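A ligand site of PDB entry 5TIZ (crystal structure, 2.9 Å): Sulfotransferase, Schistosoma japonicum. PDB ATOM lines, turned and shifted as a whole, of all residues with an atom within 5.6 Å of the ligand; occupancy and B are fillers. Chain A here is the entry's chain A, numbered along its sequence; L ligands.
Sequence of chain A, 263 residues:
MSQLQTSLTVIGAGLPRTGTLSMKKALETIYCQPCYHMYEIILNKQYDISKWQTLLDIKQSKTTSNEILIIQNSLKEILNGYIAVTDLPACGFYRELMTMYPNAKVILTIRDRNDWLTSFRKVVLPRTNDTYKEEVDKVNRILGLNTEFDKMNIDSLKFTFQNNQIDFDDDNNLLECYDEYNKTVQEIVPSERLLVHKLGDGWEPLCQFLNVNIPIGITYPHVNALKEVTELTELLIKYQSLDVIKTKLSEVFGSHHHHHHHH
O2 of the ligand sits at hydrogen-bond distance from OG of Ser 119. The backbone NH (N) of Gly 19 is in hydrogen-bond range of an oxygen (O7) of the ligand (3.0 Å). The backbone NH (N) of Leu 226 lies within hydrogen-bond range of an oxygen (O3) of the ligand, at 2.7 Å. An oxygen (O4) of the ligand is in hydrogen-bond range of the backbone NH of Arg 17. OG1 of Thr 20 sits at hydrogen-bond distance from O4 of the ligand, at 2.6 Å. OG of Ser 22 lies within hydrogen-bond range of N2 of the ligand (3.1 Å). NH1 of Arg 17 lies within salt-bridge range of O6 of the ligand, at 3.0 Å. N of Leu 21 lies within hydrogen-bond range of O5 of the ligand (2.9 Å). An oxygen (O6) of the ligand lies within hydrogen-bond range of the side-chain amide nitrogen of Asn 224, 2.7 Å away. O1 of the ligand lies within salt-bridge range of NH2 of Arg 111, at 3.0 Å. The backbone carbonyl oxygen of Pro 221 lies within hydrogen-bond range of a nitrogen (N3) of the ligand, at 2.5 Å. A ring nitrogen (NE2) of His 222 is in hydrogen-bond range of an oxygen (O10) of the ligand. N of Thr 20 lies within hydrogen-bond range of O4 of the ligand.
The backbone carbonyl oxygen (O) of Pro 221 is in hydrogen-bond range of the side-chain hydroxyl (OG) of Ser 22 (3.4 Å). The side-chain hydroxyl (OG) of Ser 119 sits at hydrogen-bond distance from the guanidinium group (NE) of Arg 17, 3.0 Å away. O of Asn 224 lies within hydrogen-bond range of NH2 of Arg 17, at 3.0 Å. The side-chain hydroxyl (OG1) of Thr 18 is in hydrogen-bond range of the backbone carbonyl oxygen (O) of Leu 15, at 2.5 Å. NH1 of Arg 111 lies within hydrogen-bond range of O of Arg 17, 2.8 Å away. The backbone NH (N) of Val 223 sits at hydrogen-bond distance from the side-chain hydroxyl (OG) of Ser 22 (2.9 Å). The side-chain amide oxygen (OD1) of Asn 224 is in hydrogen-bond range of the side-chain hydroxyl (OH) of Tyr 39 (3.0 Å). OG1 of Thr 20 lies within hydrogen-bond range of NE2 of His 37 (3.1 Å).
C of Pro 16 touches O4 of the ligand (3.98 Å). Thr 18 touches the ligand (N to O4, 3.6 Å). Leu 199 touches the ligand. CD2 of Tyr 220 touches N3 of the ligand, 3.4 Å away. O of Val 223 touches C6 of the ligand, 3.8 Å away. Ala 225 touches the ligand. Within 4 Å of the ligand: Pro 16, Arg 17, Thr 18, Gly 19, Thr 20, Leu 21, Ser 22, Arg 111, Ser 119, Leu 199, Tyr 220, Pro 221, His 222, Val 223, Asn 224, Ala 225 and Leu 226. The nearest printed residue that does not touch the ligand is Gly 200 (4.2 Å).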
ATOM      1  N   LEU A  15     -29.333  16.140   5.348  1.00  0.00           N
ATOM      2  CA  LEU A  15     -29.103  16.408   6.760  1.00  0.00           C
ATOM      3  C   LEU A  15     -27.624  16.582   7.041  1.00  0.00           C
ATOM      4  O   LEU A  15     -26.768  16.204   6.231  1.00  0.00           O
ATOM      5  CB  LEU A  15     -29.666  15.255   7.595  1.00  0.00           C
ATOM      6  CG  LEU A  15     -31.187  15.153   7.643  1.00  0.00           C
ATOM      7  CD1 LEU A  15     -31.613  13.852   8.304  1.00  0.00           C
ATOM      8  CD2 LEU A  15     -31.791  16.340   8.391  1.00  0.00           C
ATOM      9  N   PRO A  16     -27.264  17.168   8.192  1.00  0.00           N
ATOM     10  CA  PRO A  16     -25.858  17.348   8.516  1.00  0.00           C
ATOM     11  C   PRO A  16     -25.091  16.026   8.493  1.00  0.00           C
ATOM     12  O   PRO A  16     -25.632  14.969   8.821  1.00  0.00           O
ATOM     13  CB  PRO A  16     -25.882  17.956   9.933  1.00  0.00           C
ATOM     14  CG  PRO A  16     -27.285  17.775  10.422  1.00  0.00           C
ATOM     15  CD  PRO A  16     -28.148  17.782   9.209  1.00  0.00           C
ATOM     16  N   ARG A  17     -23.829  16.107   8.080  1.00  0.00           N
ATOM     17  CA  ARG A  17     -22.933  14.961   7.967  1.00  0.00           C
ATOM     18  C   ARG A  17     -23.346  13.996   6.861  1.00  0.00           C
ATOM     19  O   ARG A  17     -22.906  12.846   6.856  1.00  0.00           O
ATOM     20  CB  ARG A  17     -22.819  14.206   9.300  1.00  0.00           C
ATOM     21  CG  ARG A  17     -22.471  15.086  10.496  1.00  0.00           C
ATOM     22  CD  ARG A  17     -21.233  15.952  10.249  1.00  0.00           C
ATOM     23  NE  ARG A  17     -20.041  15.162   9.955  1.00  0.00           N
ATOM     24  CZ  ARG A  17     -18.858  15.675   9.642  1.00  0.00           C
ATOM     25  NH1 ARG A  17     -18.692  16.992   9.570  1.00  0.00           N
ATOM     26  NH2 ARG A  17     -17.825  14.872   9.401  1.00  0.00           N
ATOM     27  N   THR A  18     -24.168  14.454   5.922  1.00  0.00           N
ATOM     28  CA  THR A  18     -24.454  13.698   4.707  1.00  0.00           C
ATOM     29  C   THR A  18     -23.668  14.230   3.511  1.00  0.00           C
ATOM     30  O   THR A  18     -23.955  13.831   2.368  1.00  0.00           O
ATOM     31  CB  THR A  18     -25.951  13.733   4.395  1.00  0.00           C
ATOM     32  OG1 THR A  18     -26.374  15.066   4.084  1.00  0.00           O
ATOM     33  CG2 THR A  18     -26.762  13.212   5.581  1.00  0.00           C
ATOM     34  N   GLY A  19     -22.690  15.101   3.738  1.00  0.00           N
ATOM     35  CA  GLY A  19     -21.911  15.699   2.674  1.00  0.00           C
ATOM     36  C   GLY A  19     -22.403  17.079   2.301  1.00  0.00           C
ATOM     37  O   GLY A  19     -22.356  17.466   1.125  1.00  0.00           O
ATOM     38  N   THR A  20     -22.872  17.831   3.299  1.00  0.00           N
ATOM     39  CA  THR A  20     -23.532  19.107   3.025  1.00  0.00           C
ATOM     40  C   THR A  20     -22.530  20.220   2.716  1.00  0.00           C
ATOM     41  O   THR A  20     -22.867  21.135   1.952  1.00  0.00           O
ATOM     42  CB  THR A  20     -24.401  19.521   4.218  1.00  0.00           C
ATOM     43  OG1 THR A  20     -23.555  19.920   5.304  1.00  0.00           O
ATOM     44  CG2 THR A  20     -25.300  18.374   4.665  1.00  0.00           C
ATOM     45  N   LEU A  21     -21.329  20.174   3.284  1.00  0.00           N
ATOM     46  CA  LEU A  21     -20.340  21.188   2.960  1.00  0.00           C
ATOM     47  C   LEU A  21     -19.704  20.930   1.596  1.00  0.00           C
ATOM     48  O   LEU A  21     -19.462  21.867   0.832  1.00  0.00           O
ATOM     49  CB  LEU A  21     -19.257  21.246   4.043  1.00  0.00           C
ATOM     50  CG  LEU A  21     -18.260  22.407   3.882  1.00  0.00           C
ATOM     51  CD1 LEU A  21     -18.909  23.719   4.301  1.00  0.00           C
ATOM     52  CD2 LEU A  21     -16.982  22.165   4.681  1.00  0.00           C
ATOM     53  N   SER A  22     -19.427  19.654   1.284  1.00  0.00           N
ATOM     54  CA  SER A  22     -18.908  19.331  -0.047  1.00  0.00           C
ATOM     55  C   SER A  22     -19.925  19.685  -1.129  1.00  0.00           C
ATOM     56  O   SER A  22     -19.546  20.200  -2.187  1.00  0.00           O
ATOM     57  CB  SER A  22     -18.548  17.847  -0.118  1.00  0.00           C
ATOM     58  OG  SER A  22     -17.297  17.602   0.519  1.00  0.00           O
ATOM     59  N   HIS A  37     -25.127  27.908   4.375  1.00  0.00           N
ATOM     60  CA  HIS A  37     -24.680  26.756   5.154  1.00  0.00           C
ATOM     61  C   HIS A  37     -24.612  27.184   6.612  1.00  0.00           C
ATOM     62  O   HIS A  37     -24.537  28.380   6.926  1.00  0.00           O
ATOM     63  CB  HIS A  37     -23.306  26.261   4.669  1.00  0.00           C
ATOM     64  CG  HIS A  37     -22.915  24.922   5.218  1.00  0.00           C
ATOM     65  ND1 HIS A  37     -22.099  24.785   6.321  1.00  0.00           N
ATOM     66  CD2 HIS A  37     -23.202  23.674   4.801  1.00  0.00           C
ATOM     67  CE1 HIS A  37     -21.909  23.502   6.569  1.00  0.00           C
ATOM     68  NE2 HIS A  37     -22.566  22.801   5.666  1.00  0.00           N
ATOM     69  N   TYR A  39     -22.218  27.028   8.486  1.00  0.00           N
ATOM     70  CA  TYR A  39     -20.962  27.745   8.689  1.00  0.00           C
ATOM     71  C   TYR A  39     -21.067  29.207   8.281  1.00  0.00           C
ATOM     72  O   TYR A  39     -20.296  30.031   8.768  1.00  0.00           O
ATOM     73  CB  TYR A  39     -19.826  27.049   7.938  1.00  0.00           C
ATOM     74  CG  TYR A  39     -19.487  25.665   8.463  1.00  0.00           C
ATOM     75  CD1 TYR A  39     -20.116  25.140   9.582  1.00  0.00           C
ATOM     76  CD2 TYR A  39     -18.519  24.885   7.833  1.00  0.00           C
ATOM     77  CE1 TYR A  39     -19.791  23.882  10.057  1.00  0.00           C
ATOM     78  CE2 TYR A  39     -18.196  23.630   8.294  1.00  0.00           C
ATOM     79  CZ  TYR A  39     -18.837  23.134   9.416  1.00  0.00           C
ATOM     80  OH  TYR A  39     -18.514  21.880   9.877  1.00  0.00           O
ATOM     81  N   ASP A  87     -27.600  21.958   4.396  1.00  0.00           N
ATOM     82  CA  ASP A  87     -27.398  21.780   5.838  1.00  0.00           C
ATOM     83  C   ASP A  87     -28.556  22.379   6.620  1.00  0.00           C
ATOM     84  O   ASP A  87     -29.521  22.887   6.033  1.00  0.00           O
ATOM     85  CB  ASP A  87     -26.072  22.406   6.260  1.00  0.00           C
ATOM     86  CG  ASP A  87     -25.552  21.862   7.574  1.00  0.00           C
ATOM     87  OD1 ASP A  87     -24.800  22.585   8.261  1.00  0.00           O
ATOM     88  OD2 ASP A  87     -25.890  20.707   7.923  1.00  0.00           O
ATOM     89  N   ARG A 111     -26.288   9.084   2.832  1.00  0.00           N
ATOM     90  CA  ARG A 111     -25.203   8.137   3.024  1.00  0.00           C
ATOM     91  C   ARG A 111     -25.755   6.953   3.819  1.00  0.00           C
ATOM     92  O   ARG A 111     -26.930   6.932   4.184  1.00  0.00           O
ATOM     93  CB  ARG A 111     -24.021   8.788   3.754  1.00  0.00           C
ATOM     94  CG  ARG A 111     -24.253   8.992   5.241  1.00  0.00           C
ATOM     95  CD  ARG A 111     -23.170   9.858   5.858  1.00  0.00           C
ATOM     96  NE  ARG A 111     -21.894   9.159   5.970  1.00  0.00           N
ATOM     97  CZ  ARG A 111     -20.805   9.688   6.507  1.00  0.00           C
ATOM     98  NH1 ARG A 111     -20.837  10.923   6.988  1.00  0.00           N
ATOM     99  NH2 ARG A 111     -19.688   8.984   6.578  1.00  0.00           N
ATOM    100  N   ASP A 115     -23.216   4.736   9.108  1.00  0.00           N
ATOM    101  CA  ASP A 115     -22.065   5.638   8.975  1.00  0.00           C
ATOM    102  C   ASP A 115     -22.446   7.055   9.397  1.00  0.00           C
ATOM    103  O   ASP A 115     -21.653   7.744  10.049  1.00  0.00           O
ATOM    104  CB  ASP A 115     -21.557   5.637   7.535  1.00  0.00           C
ATOM    105  CG  ASP A 115     -21.075   4.270   7.083  1.00  0.00           C
ATOM    106  OD1 ASP A 115     -20.833   3.402   7.950  1.00  0.00           O
ATOM    107  OD2 ASP A 115     -20.943   4.063   5.862  1.00  0.00           O
ATOM    108  N   SER A 119     -20.813   9.319  12.679  1.00  0.00           N
ATOM    109  CA  SER A 119     -20.346  10.658  12.331  1.00  0.00           C
ATOM    110  C   SER A 119     -21.199  11.730  12.996  1.00  0.00           C
ATOM    111  O   SER A 119     -20.670  12.675  13.605  1.00  0.00           O
ATOM    112  CB  SER A 119     -20.349  10.833  10.821  1.00  0.00           C
ATOM    113  OG  SER A 119     -19.974  12.156  10.460  1.00  0.00           O
ATOM    114  N   LEU A 199     -23.037   9.627  -1.313  1.00  0.00           N
ATOM    115  CA  LEU A 199     -21.627   9.946  -1.110  1.00  0.00           C
ATOM    116  C   LEU A 199     -20.779   9.283  -2.176  1.00  0.00           C
ATOM    117  O   LEU A 199     -20.778   8.058  -2.319  1.00  0.00           O
ATOM    118  CB  LEU A 199     -21.172   9.510   0.279  1.00  0.00           C
ATOM    119  CG  LEU A 199     -21.263  10.464   1.480  1.00  0.00           C
ATOM    120  CD1 LEU A 199     -20.207  10.079   2.512  1.00  0.00           C
ATOM    121  CD2 LEU A 199     -21.105  11.937   1.107  1.00  0.00           C
ATOM    122  N   GLY A 200     -20.044  10.094  -2.935  1.00  0.00           N
ATOM    123  CA  GLY A 200     -19.144   9.613  -3.950  1.00  0.00           C
ATOM    124  C   GLY A 200     -19.687   9.611  -5.354  1.00  0.00           C
ATOM    125  O   GLY A 200     -18.972   9.218  -6.284  1.00  0.00           O
ATOM    126  N   TYR A 220     -14.376  16.789  -7.561  1.00  0.00           N
ATOM    127  CA  TYR A 220     -15.516  16.950  -6.669  1.00  0.00           C
ATOM    128  C   TYR A 220     -15.027  17.038  -5.220  1.00  0.00           C
ATOM    129  O   TYR A 220     -14.157  16.242  -4.817  1.00  0.00           O
ATOM    130  CB  TYR A 220     -16.486  15.777  -6.817  1.00  0.00           C
ATOM    131  CG  TYR A 220     -17.775  15.981  -6.042  1.00  0.00           C
ATOM    132  CD1 TYR A 220     -18.894  16.514  -6.668  1.00  0.00           C
ATOM    133  CD2 TYR A 220     -17.872  15.652  -4.697  1.00  0.00           C
ATOM    134  CE1 TYR A 220     -20.072  16.715  -5.969  1.00  0.00           C
ATOM    135  CE2 TYR A 220     -19.038  15.848  -3.992  1.00  0.00           C
ATOM    136  CZ  TYR A 220     -20.135  16.378  -4.636  1.00  0.00           C
ATOM    137  OH  TYR A 220     -21.307  16.571  -3.939  1.00  0.00           O
ATOM    138  N   PRO A 221     -15.529  17.982  -4.421  1.00  0.00           N
ATOM    139  CA  PRO A 221     -14.958  18.175  -3.080  1.00  0.00           C
ATOM    140  C   PRO A 221     -15.131  16.952  -2.185  1.00  0.00           C
ATOM    141  O   PRO A 221     -16.079  16.167  -2.329  1.00  0.00           O
ATOM    142  CB  PRO A 221     -15.761  19.370  -2.529  1.00  0.00           C
ATOM    143  CG  PRO A 221     -16.331  20.040  -3.720  1.00  0.00           C
ATOM    144  CD  PRO A 221     -16.586  18.960  -4.710  1.00  0.00           C
ATOM    145  N   HIS A 222     -14.186  16.807  -1.250  1.00  0.00           N
ATOM    146  CA  HIS A 222     -14.302  15.879  -0.129  1.00  0.00           C
ATOM    147  C   HIS A 222     -13.791  16.653   1.096  1.00  0.00           C
ATOM    148  O   HIS A 222     -12.661  16.487   1.544  1.00  0.00           O
ATOM    149  CB  HIS A 222     -13.515  14.593  -0.351  1.00  0.00           C
ATOM    150  CG  HIS A 222     -13.799  13.529   0.667  1.00  0.00           C
ATOM    151  ND1 HIS A 222     -13.566  12.189   0.435  1.00  0.00           N
ATOM    152  CD2 HIS A 222     -14.293  13.606   1.928  1.00  0.00           C
ATOM    153  CE1 HIS A 222     -13.905  11.489   1.501  1.00  0.00           C
ATOM    154  NE2 HIS A 222     -14.348  12.328   2.427  1.00  0.00           N
ATOM    155  N   VAL A 223     -14.659  17.520   1.633  1.00  0.00           N
ATOM    156  CA  VAL A 223     -14.308  18.417   2.716  1.00  0.00           C
ATOM    157  C   VAL A 223     -15.147  18.071   3.942  1.00  0.00           C
ATOM    158  O   VAL A 223     -16.129  17.342   3.863  1.00  0.00           O
ATOM    159  CB  VAL A 223     -14.487  19.903   2.336  1.00  0.00           C
ATOM    160  CG1 VAL A 223     -13.508  20.287   1.237  1.00  0.00           C
ATOM    161  CG2 VAL A 223     -15.924  20.171   1.883  1.00  0.00           C
ATOM    162  N   ASN A 224     -14.734  18.622   5.086  1.00  0.00           N
ATOM    163  CA  ASN A 224     -15.447  18.445   6.346  1.00  0.00           C
ATOM    164  C   ASN A 224     -15.397  16.994   6.821  1.00  0.00           C
ATOM    165  O   ASN A 224     -16.349  16.486   7.406  1.00  0.00           O
ATOM    166  CB  ASN A 224     -16.898  18.927   6.226  1.00  0.00           C
ATOM    167  CG  ASN A 224     -17.378  19.633   7.470  1.00  0.00           C
ATOM    168  OD1 ASN A 224     -16.616  20.349   8.125  1.00  0.00           O
ATOM    169  ND2 ASN A 224     -18.645  19.441   7.813  1.00  0.00           N
ATOM    170  N   ALA A 225     -14.267  16.335   6.578  1.00  0.00           N
ATOM    171  CA  ALA A 225     -14.101  14.963   7.016  1.00  0.00           C
ATOM    172  C   ALA A 225     -13.815  14.898   8.516  1.00  0.00           C
ATOM    173  O   ALA A 225     -13.363  15.875   9.126  1.00  0.00           O
ATOM    174  CB  ALA A 225     -12.980  14.281   6.234  1.00  0.00           C
ATOM    175  N   LEU A 226     -14.079  13.729   9.100  1.00  0.00           N
ATOM    176  CA  LEU A 226     -13.859  13.527  10.533  1.00  0.00           C
ATOM    177  C   LEU A 226     -12.479  14.011  10.952  1.00  0.00           C
ATOM    178  O   LEU A 226     -12.331  14.774  11.921  1.00  0.00           O
ATOM    179  CB  LEU A 226     -14.047  12.044  10.868  1.00  0.00           C
ATOM    180  CG  LEU A 226     -13.855  11.613  12.323  1.00  0.00           C
ATOM    181  CD1 LEU A 226     -15.153  11.768  13.107  1.00  0.00           C
ATOM    182  CD2 LEU A 226     -13.362  10.175  12.382  1.00  0.00           C
ATOM    183  N   LYS A 227     -11.446  13.551  10.244  1.00  0.00           N
ATOM    184  CA  LYS A 227     -10.067  13.938  10.560  1.00  0.00           C
ATOM    185  C   LYS A 227      -9.941  15.450  10.742  1.00  0.00           C
ATOM    186  O   LYS A 227      -9.417  15.927  11.751  1.00  0.00           O
ATOM    187  CB  LYS A 227      -9.138  13.451   9.444  1.00  0.00           C
ATOM    188  CG  LYS A 227      -7.758  14.098   9.342  1.00  0.00           C
ATOM    189  CD  LYS A 227      -6.748  13.533  10.330  1.00  0.00           C
ATOM    190  CE  LYS A 227      -5.335  13.665   9.780  1.00  0.00           C
ATOM    191  NZ  LYS A 227      -4.312  13.088  10.683  1.00  0.00           N
HETATM  192  P1  LIG L   1     -17.186  11.424   7.920  1.00  0.00           P
HETATM  193  O1  LIG L   1     -17.036   9.953   7.647  1.00  0.00           O
HETATM  194  O2  LIG L   1     -17.721  11.621   9.273  1.00  0.00           O
HETATM  195  O3  LIG L   1     -15.866  12.098   7.793  1.00  0.00           O
HETATM  196  P2  LIG L   1     -21.056  17.423   6.133  1.00  0.00           P
HETATM  197  O4  LIG L   1     -22.534  17.621   5.891  1.00  0.00           O
HETATM  198  O5  LIG L   1     -20.266  18.294   5.181  1.00  0.00           O
HETATM  199  O6  LIG L   1     -20.749  17.786   7.561  1.00  0.00           O
HETATM  200  O7  LIG L   1     -20.639  15.822   5.852  1.00  0.00           O
HETATM  201  C1  LIG L   1     -19.309  15.425   6.059  1.00  0.00           C
HETATM  202  C2  LIG L   1     -19.241  13.851   5.961  1.00  0.00           C
HETATM  203  O8  LIG L   1     -19.461  13.440   4.490  1.00  0.00           O
HETATM  204  C3  LIG L   1     -18.086  13.390   6.288  1.00  0.00           C
HETATM  205  O9  LIG L   1     -18.247  12.046   6.812  1.00  0.00           O
HETATM  206  C4  LIG L   1     -17.245  13.347   4.855  1.00  0.00           C
HETATM  207  O10 LIG L   1     -16.058  12.488   4.992  1.00  0.00           O
HETATM  208  C5  LIG L   1     -18.080  12.830   4.043  1.00  0.00           C
HETATM  209  N1  LIG L   1     -17.812  13.118   2.599  1.00  0.00           N
HETATM  210  C6  LIG L   1     -18.039  14.417   2.336  1.00  0.00           C
HETATM  211  N2  LIG L   1     -17.781  14.616   1.043  1.00  0.00           N
HETATM  212  C7  LIG L   1     -17.407  13.447   0.504  1.00  0.00           C
HETATM  213  C8  LIG L   1     -17.045  13.107  -0.761  1.00  0.00           C
HETATM  214  N3  LIG L   1     -16.889  13.772  -2.023  1.00  0.00           N
HETATM  215  N4  LIG L   1     -16.711  11.879  -1.041  1.00  0.00           N
HETATM  216  C9  LIG L   1     -16.730  10.933  -0.059  1.00  0.00           C
HETATM  217  N5  LIG L   1     -17.087  11.270   1.189  1.00  0.00           N
HETATM  218  C10 LIG L   1     -17.423  12.526   1.463  1.00  0.00           C
